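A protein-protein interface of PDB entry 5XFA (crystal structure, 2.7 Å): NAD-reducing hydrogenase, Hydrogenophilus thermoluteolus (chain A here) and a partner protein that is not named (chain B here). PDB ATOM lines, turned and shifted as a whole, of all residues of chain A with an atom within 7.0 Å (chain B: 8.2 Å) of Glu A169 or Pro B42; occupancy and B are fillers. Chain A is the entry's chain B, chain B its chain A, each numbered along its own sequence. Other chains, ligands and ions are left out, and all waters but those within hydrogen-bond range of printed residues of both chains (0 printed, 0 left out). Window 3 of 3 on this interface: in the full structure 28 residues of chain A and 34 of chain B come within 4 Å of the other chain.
Glu A169 touches Pro B42.
Val A172 touches Ala B48 (CG1 to CB, 3.9 Å).
Pro B42 touches Thr A185 (CB to OG1, 3.5 Å).
Pro B43 touches Thr A185 (N to O, 3.8 Å).
Ala A187 touches Pro B43.
Of the 19 printed residues of chain A, 4 touch a printed residue of chain B.
Hydrophobic or aromatic side chains of chain A within 4 Å of the printed part of chain B: Val A172.
Along chain A the printed residues that touch a printed residue of chain B span positions 169 to 187.
Of the 18 printed residues of chain B, 5 touch a printed residue of chain A.
Hydrophobic or aromatic side chains of chain B within 4 Å of the printed part of chain A: Pro B42, Pro B43 and Ala B48.
The backbone carbonyl oxygen (O) of Thr A185 lies within hydrogen-bond range of the backbone NH (N) of Gly B44, 3.0 Å away.
NH1 of Arg B7 is in salt-bridge range of OE1 of Glu A169 (2.7 Å).
Glu A169 touches just these residues of chain B: Arg B7 (2.7 Å) and Pro B42 (3.5 Å).
No residue of chain B comes within 4 Å of Ala A170.
Of the printed residues of chain B, Val A172 touches Ala B48 (3.9 Å).
Printed residues of chain A within 4 Å of Arg B7: Glu A169 (2.7 Å).
Printed residues of chain A within 4 Å of Pro B43: Thr A185 (3.8 Å) and Ala A187 (3.9 Å).
Printed residues of chain A within 4 Å of Gly B44: Thr A185 (3.0 Å).
Printed residues of chain A within 4 Å of Ala B48: Val A172.
The nearest residue of chain B that does not touch Glu A169 is Ser B40 (5.0 Å).
The nearest residue of chain A that does not touch Pro B42 is Ser A186 (5.5 Å).
N of Thr A185 lies within hydrogen-bond range of O of Ala A170, at 2.8 Å.
O of Glu A169 sits at hydrogen-bond distance from OG1 of Thr A185 (2.8 Å).
The side-chain carboxylate (OE2) of Glu B45 is in salt-bridge range of the guanidinium group (NH2) of Arg B7, 3.0 Å away.
The backbone NH (N) of Glu A169 is in hydrogen-bond range of the backbone carbonyl oxygen (O) of Ser A163, 3.1 Å away.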
ATOM      1  N   VAL A 160      11.593  11.454 -24.326  1.00  0.00           N
ATOM      2  CA  VAL A 160      12.345  12.682 -24.502  1.00  0.00           C
ATOM      3  C   VAL A 160      13.293  12.546 -25.689  1.00  0.00           C
ATOM      4  O   VAL A 160      13.193  13.310 -26.659  1.00  0.00           O
ATOM      5  CB  VAL A 160      13.155  13.051 -23.241  1.00  0.00           C
ATOM      6  CG1 VAL A 160      14.148  14.179 -23.553  1.00  0.00           C
ATOM      7  CG2 VAL A 160      12.226  13.450 -22.090  1.00  0.00           C
ATOM      8  N   ALA A 162      13.608  10.380 -28.102  1.00  0.00           N
ATOM      9  CA  ALA A 162      12.924  10.216 -29.370  1.00  0.00           C
ATOM     10  C   ALA A 162      12.502  11.549 -29.967  1.00  0.00           C
ATOM     11  O   ALA A 162      12.625  11.749 -31.176  1.00  0.00           O
ATOM     12  CB  ALA A 162      11.722   9.280 -29.204  1.00  0.00           C
ATOM     13  N   SER A 163      12.004  12.453 -29.129  1.00  0.00           N
ATOM     14  CA  SER A 163      11.438  13.699 -29.617  1.00  0.00           C
ATOM     15  C   SER A 163      12.533  14.721 -29.993  1.00  0.00           C
ATOM     16  O   SER A 163      12.391  15.495 -30.957  1.00  0.00           O
ATOM     17  CB  SER A 163      10.476  14.279 -28.588  1.00  0.00           C
ATOM     18  OG  SER A 163       9.488  15.103 -29.200  1.00  0.00           O
ATOM     19  N   LEU A 164      13.618  14.744 -29.225  1.00  0.00           N
ATOM     20  CA  LEU A 164      14.778  15.578 -29.572  1.00  0.00           C
ATOM     21  C   LEU A 164      15.263  15.133 -30.924  1.00  0.00           C
ATOM     22  O   LEU A 164      15.380  15.943 -31.829  1.00  0.00           O
ATOM     23  CB  LEU A 164      15.894  15.453 -28.541  1.00  0.00           C
ATOM     24  CG  LEU A 164      15.609  15.804 -27.076  1.00  0.00           C
ATOM     25  CD1 LEU A 164      16.887  15.772 -26.256  1.00  0.00           C
ATOM     26  CD2 LEU A 164      14.922  17.160 -26.900  1.00  0.00           C
ATOM     27  N   ALA A 165      15.476  13.835 -31.087  1.00  0.00           N
ATOM     28  CA  ALA A 165      16.031  13.296 -32.334  1.00  0.00           C
ATOM     29  C   ALA A 165      15.211  13.578 -33.593  1.00  0.00           C
ATOM     30  O   ALA A 165      15.783  13.753 -34.650  1.00  0.00           O
ATOM     31  CB  ALA A 165      16.273  11.806 -32.220  1.00  0.00           C
ATOM     32  N   GLU A 166      13.887  13.624 -33.498  1.00  0.00           N
ATOM     33  CA  GLU A 166      13.085  13.878 -34.692  1.00  0.00           C
ATOM     34  C   GLU A 166      12.670  15.330 -34.788  1.00  0.00           C
ATOM     35  O   GLU A 166      11.966  15.707 -35.726  1.00  0.00           O
ATOM     36  CB  GLU A 166      11.882  12.960 -34.763  1.00  0.00           C
ATOM     37  CG  GLU A 166      10.703  13.391 -33.926  1.00  0.00           C
ATOM     38  CD  GLU A 166       9.807  12.226 -33.545  1.00  0.00           C
ATOM     39  OE1 GLU A 166       9.538  11.356 -34.421  1.00  0.00           O
ATOM     40  OE2 GLU A 166       9.420  12.191 -32.348  1.00  0.00           O
ATOM     41  N   GLY A 167      13.122  16.139 -33.828  1.00  0.00           N
ATOM     42  CA  GLY A 167      13.107  17.599 -33.960  1.00  0.00           C
ATOM     43  C   GLY A 167      11.948  18.318 -33.290  1.00  0.00           C
ATOM     44  O   GLY A 167      11.908  19.556 -33.268  1.00  0.00           O
ATOM     45  N   LYS A 168      11.017  17.557 -32.731  1.00  0.00           N
ATOM     46  CA  LYS A 168       9.827  18.141 -32.138  1.00  0.00           C
ATOM     47  C   LYS A 168      10.085  18.731 -30.744  1.00  0.00           C
ATOM     48  O   LYS A 168       9.399  19.679 -30.347  1.00  0.00           O
ATOM     49  CB  LYS A 168       8.724  17.095 -32.061  1.00  0.00           C
ATOM     50  CG  LYS A 168       8.354  16.459 -33.399  1.00  0.00           C
ATOM     51  CD  LYS A 168       7.697  17.436 -34.366  1.00  0.00           C
ATOM     52  CE  LYS A 168       6.854  16.702 -35.400  1.00  0.00           C
ATOM     53  NZ  LYS A 168       5.495  16.297 -34.876  1.00  0.00           N
ATOM     54  N   GLU A 169      11.047  18.172 -30.004  1.00  0.00           N
ATOM     55  CA  GLU A 169      11.406  18.680 -28.671  1.00  0.00           C
ATOM     56  C   GLU A 169      10.203  18.849 -27.748  1.00  0.00           C
ATOM     57  O   GLU A 169      10.125  19.808 -26.985  1.00  0.00           O
ATOM     58  CB  GLU A 169      12.090  20.034 -28.775  1.00  0.00           C
ATOM     59  CG  GLU A 169      13.127  20.166 -29.871  1.00  0.00           C
ATOM     60  CD  GLU A 169      13.778  21.538 -29.852  1.00  0.00           C
ATOM     61  OE1 GLU A 169      15.030  21.589 -29.927  1.00  0.00           O
ATOM     62  OE2 GLU A 169      13.046  22.559 -29.764  1.00  0.00           O
ATOM     63  N   ALA A 170       9.271  17.905 -27.801  1.00  0.00           N
ATOM     64  CA  ALA A 170       7.996  18.075 -27.117  1.00  0.00           C
ATOM     65  C   ALA A 170       8.082  17.842 -25.629  1.00  0.00           C
ATOM     66  O   ALA A 170       7.273  18.383 -24.892  1.00  0.00           O
ATOM     67  CB  ALA A 170       6.949  17.169 -27.724  1.00  0.00           C
ATOM     68  N   LEU A 171       9.051  17.052 -25.177  1.00  0.00           N
ATOM     69  CA  LEU A 171       9.076  16.623 -23.775  1.00  0.00           C
ATOM     70  C   LEU A 171      10.391  16.906 -23.053  1.00  0.00           C
ATOM     71  O   LEU A 171      11.430  17.164 -23.677  1.00  0.00           O
ATOM     72  CB  LEU A 171       8.744  15.141 -23.690  1.00  0.00           C
ATOM     73  CG  LEU A 171       7.427  14.766 -24.386  1.00  0.00           C
ATOM     74  CD1 LEU A 171       7.461  13.338 -24.911  1.00  0.00           C
ATOM     75  CD2 LEU A 171       6.247  14.953 -23.464  1.00  0.00           C
ATOM     76  N   VAL A 172      10.337  16.840 -21.725  1.00  0.00           N
ATOM     77  CA  VAL A 172      11.517  17.069 -20.905  1.00  0.00           C
ATOM     78  C   VAL A 172      11.235  16.616 -19.499  1.00  0.00           C
ATOM     79  O   VAL A 172      10.123  16.710 -19.031  1.00  0.00           O
ATOM     80  CB  VAL A 172      11.934  18.557 -20.886  1.00  0.00           C
ATOM     81  CG1 VAL A 172      10.880  19.414 -20.183  1.00  0.00           C
ATOM     82  CG2 VAL A 172      13.299  18.731 -20.226  1.00  0.00           C
ATOM     83  N   ALA A 184       5.722  18.467 -20.509  1.00  0.00           N
ATOM     84  CA  ALA A 184       5.607  18.949 -21.871  1.00  0.00           C
ATOM     85  C   ALA A 184       6.396  20.246 -21.982  1.00  0.00           C
ATOM     86  O   ALA A 184       6.380  21.037 -21.049  1.00  0.00           O
ATOM     87  CB  ALA A 184       4.150  19.190 -22.179  1.00  0.00           C
ATOM     88  N   THR A 185       7.077  20.488 -23.094  1.00  0.00           N
ATOM     89  CA  THR A 185       7.898  21.737 -23.229  1.00  0.00           C
ATOM     90  C   THR A 185       7.118  22.965 -23.674  1.00  0.00           C
ATOM     91  O   THR A 185       7.723  24.003 -23.958  1.00  0.00           O
ATOM     92  CB  THR A 185       9.045  21.621 -24.240  1.00  0.00           C
ATOM     93  OG1 THR A 185       8.497  21.537 -25.563  1.00  0.00           O
ATOM     94  CG2 THR A 185       9.900  20.432 -23.945  1.00  0.00           C
ATOM     95  N   SER A 186       5.794  22.842 -23.763  1.00  0.00           N
ATOM     96  CA  SER A 186       4.954  23.940 -24.181  1.00  0.00           C
ATOM     97  C   SER A 186       4.880  24.971 -23.061  1.00  0.00           C
ATOM     98  O   SER A 186       5.018  24.654 -21.878  1.00  0.00           O
ATOM     99  CB  SER A 186       3.558  23.422 -24.527  1.00  0.00           C
ATOM    100  OG  SER A 186       3.007  22.693 -23.437  1.00  0.00           O
ATOM    101  N   ALA A 187       4.646  26.216 -23.439  1.00  0.00           N
ATOM    102  CA  ALA A 187       4.543  27.278 -22.453  1.00  0.00           C
ATOM    103  C   ALA A 187       3.441  26.983 -21.427  1.00  0.00           C
ATOM    104  O   ALA A 187       3.598  27.296 -20.245  1.00  0.00           O
ATOM    105  CB  ALA A 187       4.312  28.624 -23.136  1.00  0.00           C
ATOM    106  N   THR A 194       2.297  21.391 -27.544  1.00  0.00           N
ATOM    107  CA  THR A 194       3.581  21.070 -28.145  1.00  0.00           C
ATOM    108  C   THR A 194       3.353  20.584 -29.570  1.00  0.00           C
ATOM    109  O   THR A 194       2.228  20.390 -29.997  1.00  0.00           O
ATOM    110  CB  THR A 194       4.292  19.921 -27.419  1.00  0.00           C
ATOM    111  OG1 THR A 194       3.658  18.701 -27.772  1.00  0.00           O
ATOM    112  CG2 THR A 194       4.285  20.096 -25.899  1.00  0.00           C
ATOM    113  N   ALA A 195       4.434  20.345 -30.291  1.00  0.00           N
ATOM    114  CA  ALA A 195       4.359  19.874 -31.673  1.00  0.00           C
ATOM    115  C   ALA A 195       4.237  18.359 -31.761  1.00  0.00           C
ATOM    116  O   ALA A 195       4.322  17.795 -32.851  1.00  0.00           O
ATOM    117  CB  ALA A 195       5.611  20.335 -32.433  1.00  0.00           C
ATOM    118  N   LEU A 196       4.105  17.683 -30.620  1.00  0.00           N
ATOM    119  CA  LEU A 196       3.955  16.225 -30.597  1.00  0.00           C
ATOM    120  C   LEU A 196       2.789  15.765 -31.494  1.00  0.00           C
ATOM    121  O   LEU A 196       1.709  16.337 -31.440  1.00  0.00           O
ATOM    122  CB  LEU A 196       3.699  15.780 -29.169  1.00  0.00           C
ATOM    123  CG  LEU A 196       3.455  14.308 -28.857  1.00  0.00           C
ATOM    124  CD1 LEU A 196       4.603  13.434 -29.320  1.00  0.00           C
ATOM    125  CD2 LEU A 196       3.273  14.167 -27.356  1.00  0.00           C
ATOM    126  N   GLN B   6      25.441  19.215 -26.850  1.00  0.00           N
ATOM    127  CA  GLN B   6      24.323  19.205 -27.838  1.00  0.00           C
ATOM    128  C   GLN B   6      23.219  20.203 -27.463  1.00  0.00           C
ATOM    129  O   GLN B   6      22.821  21.028 -28.293  1.00  0.00           O
ATOM    130  CB  GLN B   6      23.749  17.790 -27.981  1.00  0.00           C
ATOM    131  CG  GLN B   6      24.806  16.734 -28.287  1.00  0.00           C
ATOM    132  CD  GLN B   6      24.341  15.691 -29.295  1.00  0.00           C
ATOM    133  OE1 GLN B   6      24.078  16.010 -30.459  1.00  0.00           O
ATOM    134  NE2 GLN B   6      24.259  14.435 -28.859  1.00  0.00           N
ATOM    135  N   ARG B   7      22.747  20.131 -26.215  1.00  0.00           N
ATOM    136  CA  ARG B   7      21.655  20.996 -25.718  1.00  0.00           C
ATOM    137  C   ARG B   7      22.139  22.182 -24.878  1.00  0.00           C
ATOM    138  O   ARG B   7      21.388  22.695 -24.041  1.00  0.00           O
ATOM    139  CB  ARG B   7      20.678  20.175 -24.864  1.00  0.00           C
ATOM    140  CG  ARG B   7      19.971  19.041 -25.591  1.00  0.00           C
ATOM    141  CD  ARG B   7      19.059  19.540 -26.707  1.00  0.00           C
ATOM    142  NE  ARG B   7      17.891  20.278 -26.229  1.00  0.00           N
ATOM    143  CZ  ARG B   7      16.988  20.851 -27.025  1.00  0.00           C
ATOM    144  NH1 ARG B   7      17.115  20.776 -28.340  1.00  0.00           N
ATOM    145  NH2 ARG B   7      15.948  21.506 -26.514  1.00  0.00           N
ATOM    146  N   LEU B  32       9.587  33.588 -19.699  1.00  0.00           N
ATOM    147  CA  LEU B  32      10.009  32.340 -20.336  1.00  0.00           C
ATOM    148  C   LEU B  32      10.071  32.458 -21.864  1.00  0.00           C
ATOM    149  O   LEU B  32      10.961  31.894 -22.490  1.00  0.00           O
ATOM    150  CB  LEU B  32       9.073  31.182 -19.956  1.00  0.00           C
ATOM    151  CG  LEU B  32       8.998  30.751 -18.485  1.00  0.00           C
ATOM    152  CD1 LEU B  32       7.928  29.684 -18.267  1.00  0.00           C
ATOM    153  CD2 LEU B  32      10.347  30.242 -17.998  1.00  0.00           C
ATOM    154  N   ALA B  33       9.117  33.170 -22.460  1.00  0.00           N
ATOM    155  CA  ALA B  33       9.109  33.385 -23.910  1.00  0.00           C
ATOM    156  C   ALA B  33      10.329  34.202 -24.362  1.00  0.00           C
ATOM    157  O   ALA B  33      10.871  33.976 -25.445  1.00  0.00           O
ATOM    158  CB  ALA B  33       7.814  34.064 -24.345  1.00  0.00           C
ATOM    159  N   LEU B  35      13.262  34.232 -22.875  1.00  0.00           N
ATOM    160  CA  LEU B  35      14.432  33.368 -22.746  1.00  0.00           C
ATOM    161  C   LEU B  35      14.425  32.258 -23.802  1.00  0.00           C
ATOM    162  O   LEU B  35      15.471  31.801 -24.272  1.00  0.00           O
ATOM    163  CB  LEU B  35      14.525  32.774 -21.328  1.00  0.00           C
ATOM    164  CG  LEU B  35      14.704  33.770 -20.166  1.00  0.00           C
ATOM    165  CD1 LEU B  35      14.828  33.059 -18.830  1.00  0.00           C
ATOM    166  CD2 LEU B  35      15.899  34.694 -20.374  1.00  0.00           C
ATOM    167  N   SER B  36      13.236  31.820 -24.158  1.00  0.00           N
ATOM    168  CA  SER B  36      13.096  30.768 -25.139  1.00  0.00           C
ATOM    169  C   SER B  36      13.667  31.231 -26.475  1.00  0.00           C
ATOM    170  O   SER B  36      14.352  30.469 -27.150  1.00  0.00           O
ATOM    171  CB  SER B  36      11.624  30.348 -25.263  1.00  0.00           C
ATOM    172  OG  SER B  36      11.447  29.404 -26.304  1.00  0.00           O
ATOM    173  N   THR B  37      13.392  32.478 -26.844  1.00  0.00           N
ATOM    174  CA  THR B  37      13.965  33.060 -28.067  1.00  0.00           C
ATOM    175  C   THR B  37      15.467  33.251 -27.908  1.00  0.00           C
ATOM    176  O   THR B  37      16.266  32.772 -28.732  1.00  0.00           O
ATOM    177  CB  THR B  37      13.339  34.427 -28.397  1.00  0.00           C
ATOM    178  OG1 THR B  37      11.915  34.350 -28.247  1.00  0.00           O
ATOM    179  CG2 THR B  37      13.699  34.851 -29.826  1.00  0.00           C
ATOM    180  N   PHE B  39      17.518  31.783 -26.019  1.00  0.00           N
ATOM    181  CA  PHE B  39      18.321  30.579 -25.877  1.00  0.00           C
ATOM    182  C   PHE B  39      17.976  29.409 -26.794  1.00  0.00           C
ATOM    183  O   PHE B  39      18.612  28.363 -26.697  1.00  0.00           O
ATOM    184  CB  PHE B  39      18.334  30.142 -24.418  1.00  0.00           C
ATOM    185  CG  PHE B  39      19.126  31.055 -23.543  1.00  0.00           C
ATOM    186  CD1 PHE B  39      20.507  30.930 -23.466  1.00  0.00           C
ATOM    187  CD2 PHE B  39      18.511  32.075 -22.841  1.00  0.00           C
ATOM    188  CE1 PHE B  39      21.258  31.797 -22.686  1.00  0.00           C
ATOM    189  CE2 PHE B  39      19.252  32.938 -22.043  1.00  0.00           C
ATOM    190  CZ  PHE B  39      20.626  32.802 -21.968  1.00  0.00           C
ATOM    191  N   SER B  40      17.024  29.588 -27.707  1.00  0.00           N
ATOM    192  CA  SER B  40      16.599  28.510 -28.624  1.00  0.00           C
ATOM    193  C   SER B  40      16.174  27.236 -27.885  1.00  0.00           C
ATOM    194  O   SER B  40      16.460  26.124 -28.326  1.00  0.00           O
ATOM    195  CB  SER B  40      17.687  28.195 -29.644  1.00  0.00           C
ATOM    196  OG  SER B  40      17.842  29.286 -30.531  1.00  0.00           O
ATOM    197  N   LEU B  41      15.497  27.408 -26.755  1.00  0.00           N
ATOM    198  CA  LEU B  41      14.976  26.290 -26.018  1.00  0.00           C
ATOM    199  C   LEU B  41      13.498  26.539 -25.812  1.00  0.00           C
ATOM    200  O   LEU B  41      13.104  27.679 -25.560  1.00  0.00           O
ATOM    201  CB  LEU B  41      15.683  26.156 -24.665  1.00  0.00           C
ATOM    202  CG  LEU B  41      17.150  25.712 -24.694  1.00  0.00           C
ATOM    203  CD1 LEU B  41      17.712  25.564 -23.280  1.00  0.00           C
ATOM    204  CD2 LEU B  41      17.304  24.413 -25.464  1.00  0.00           C
ATOM    205  N   PRO B  42      12.672  25.476 -25.904  1.00  0.00           N
ATOM    206  CA  PRO B  42      11.246  25.687 -25.688  1.00  0.00           C
ATOM    207  C   PRO B  42      10.971  26.107 -24.252  1.00  0.00           C
ATOM    208  O   PRO B  42      11.627  25.615 -23.331  1.00  0.00           O
ATOM    209  CB  PRO B  42      10.622  24.320 -25.982  1.00  0.00           C
ATOM    210  CG  PRO B  42      11.678  23.517 -26.647  1.00  0.00           C
ATOM    211  CD  PRO B  42      12.980  24.056 -26.147  1.00  0.00           C
ATOM    212  N   PRO B  43       9.997  27.002 -24.059  1.00  0.00           N
ATOM    213  CA  PRO B  43       9.705  27.604 -22.754  1.00  0.00           C
ATOM    214  C   PRO B  43       9.665  26.635 -21.555  1.00  0.00           C
ATOM    215  O   PRO B  43      10.188  26.966 -20.494  1.00  0.00           O
ATOM    216  CB  PRO B  43       8.330  28.237 -22.963  1.00  0.00           C
ATOM    217  CG  PRO B  43       8.244  28.482 -24.431  1.00  0.00           C
ATOM    218  CD  PRO B  43       9.005  27.378 -25.080  1.00  0.00           C
ATOM    219  N   GLY B  44       9.037  25.472 -21.719  1.00  0.00           N
ATOM    220  CA  GLY B  44       8.974  24.466 -20.661  1.00  0.00           C
ATOM    221  C   GLY B  44      10.302  23.785 -20.327  1.00  0.00           C
ATOM    222  O   GLY B  44      10.529  23.389 -19.192  1.00  0.00           O
ATOM    223  N   GLU B  45      11.182  23.643 -21.311  1.00  0.00           N
ATOM    224  CA  GLU B  45      12.545  23.175 -21.046  1.00  0.00           C
ATOM    225  C   GLU B  45      13.286  24.142 -20.095  1.00  0.00           C
ATOM    226  O   GLU B  45      13.981  23.729 -19.150  1.00  0.00           O
ATOM    227  CB  GLU B  45      13.326  22.997 -22.349  1.00  0.00           C
ATOM    228  CG  GLU B  45      14.638  22.254 -22.145  1.00  0.00           C
ATOM    229  CD  GLU B  45      15.124  21.482 -23.364  1.00  0.00           C
ATOM    230  OE1 GLU B  45      14.296  20.878 -24.095  1.00  0.00           O
ATOM    231  OE2 GLU B  45      16.359  21.456 -23.577  1.00  0.00           O
ATOM    232  N   ILE B  46      13.093  25.431 -20.335  1.00  0.00           N
ATOM    233  CA  ILE B  46      13.640  26.462 -19.469  1.00  0.00           C
ATOM    234  C   ILE B  46      13.002  26.383 -18.080  1.00  0.00           C
ATOM    235  O   ILE B  46      13.701  26.354 -17.069  1.00  0.00           O
ATOM    236  CB  ILE B  46      13.498  27.855 -20.125  1.00  0.00           C
ATOM    237  CG1 ILE B  46      14.470  27.927 -21.309  1.00  0.00           C
ATOM    238  CG2 ILE B  46      13.799  28.970 -19.138  1.00  0.00           C
ATOM    239  CD1 ILE B  46      14.385  29.190 -22.129  1.00  0.00           C
ATOM    240  N   ALA B  47      11.676  26.304 -18.040  1.00  0.00           N
ATOM    241  CA  ALA B  47      10.944  26.099 -16.787  1.00  0.00           C
ATOM    242  C   ALA B  47      11.480  24.917 -15.998  1.00  0.00           C
ATOM    243  O   ALA B  47      11.655  24.995 -14.772  1.00  0.00           O
ATOM    244  CB  ALA B  47       9.472  25.888 -17.071  1.00  0.00           C
ATOM    245  N   ALA B  48      11.747  23.830 -16.715  1.00  0.00           N
ATOM    246  CA  ALA B  48      12.195  22.573 -16.116  1.00  0.00           C
ATOM    247  C   ALA B  48      13.582  22.686 -15.481  1.00  0.00           C
ATOM    248  O   ALA B  48      13.819  22.183 -14.368  1.00  0.00           O
ATOM    249  CB  ALA B  48      12.206  21.496 -17.181  1.00  0.00           C
ATOM    250  N   THR B  49      14.492  23.331 -16.220  1.00  0.00           N
ATOM    251  CA  THR B  49      15.822  23.673 -15.730  1.00  0.00           C
ATOM    252  C   THR B  49      15.710  24.539 -14.466  1.00  0.00           C
ATOM    253  O   THR B  49      16.265  24.207 -13.413  1.00  0.00           O
ATOM    254  CB  THR B  49      16.599  24.443 -16.805  1.00  0.00           C
ATOM    255  OG1 THR B  49      16.731  23.624 -17.973  1.00  0.00           O
ATOM    256  CG2 THR B  49      17.968  24.853 -16.310  1.00  0.00           C
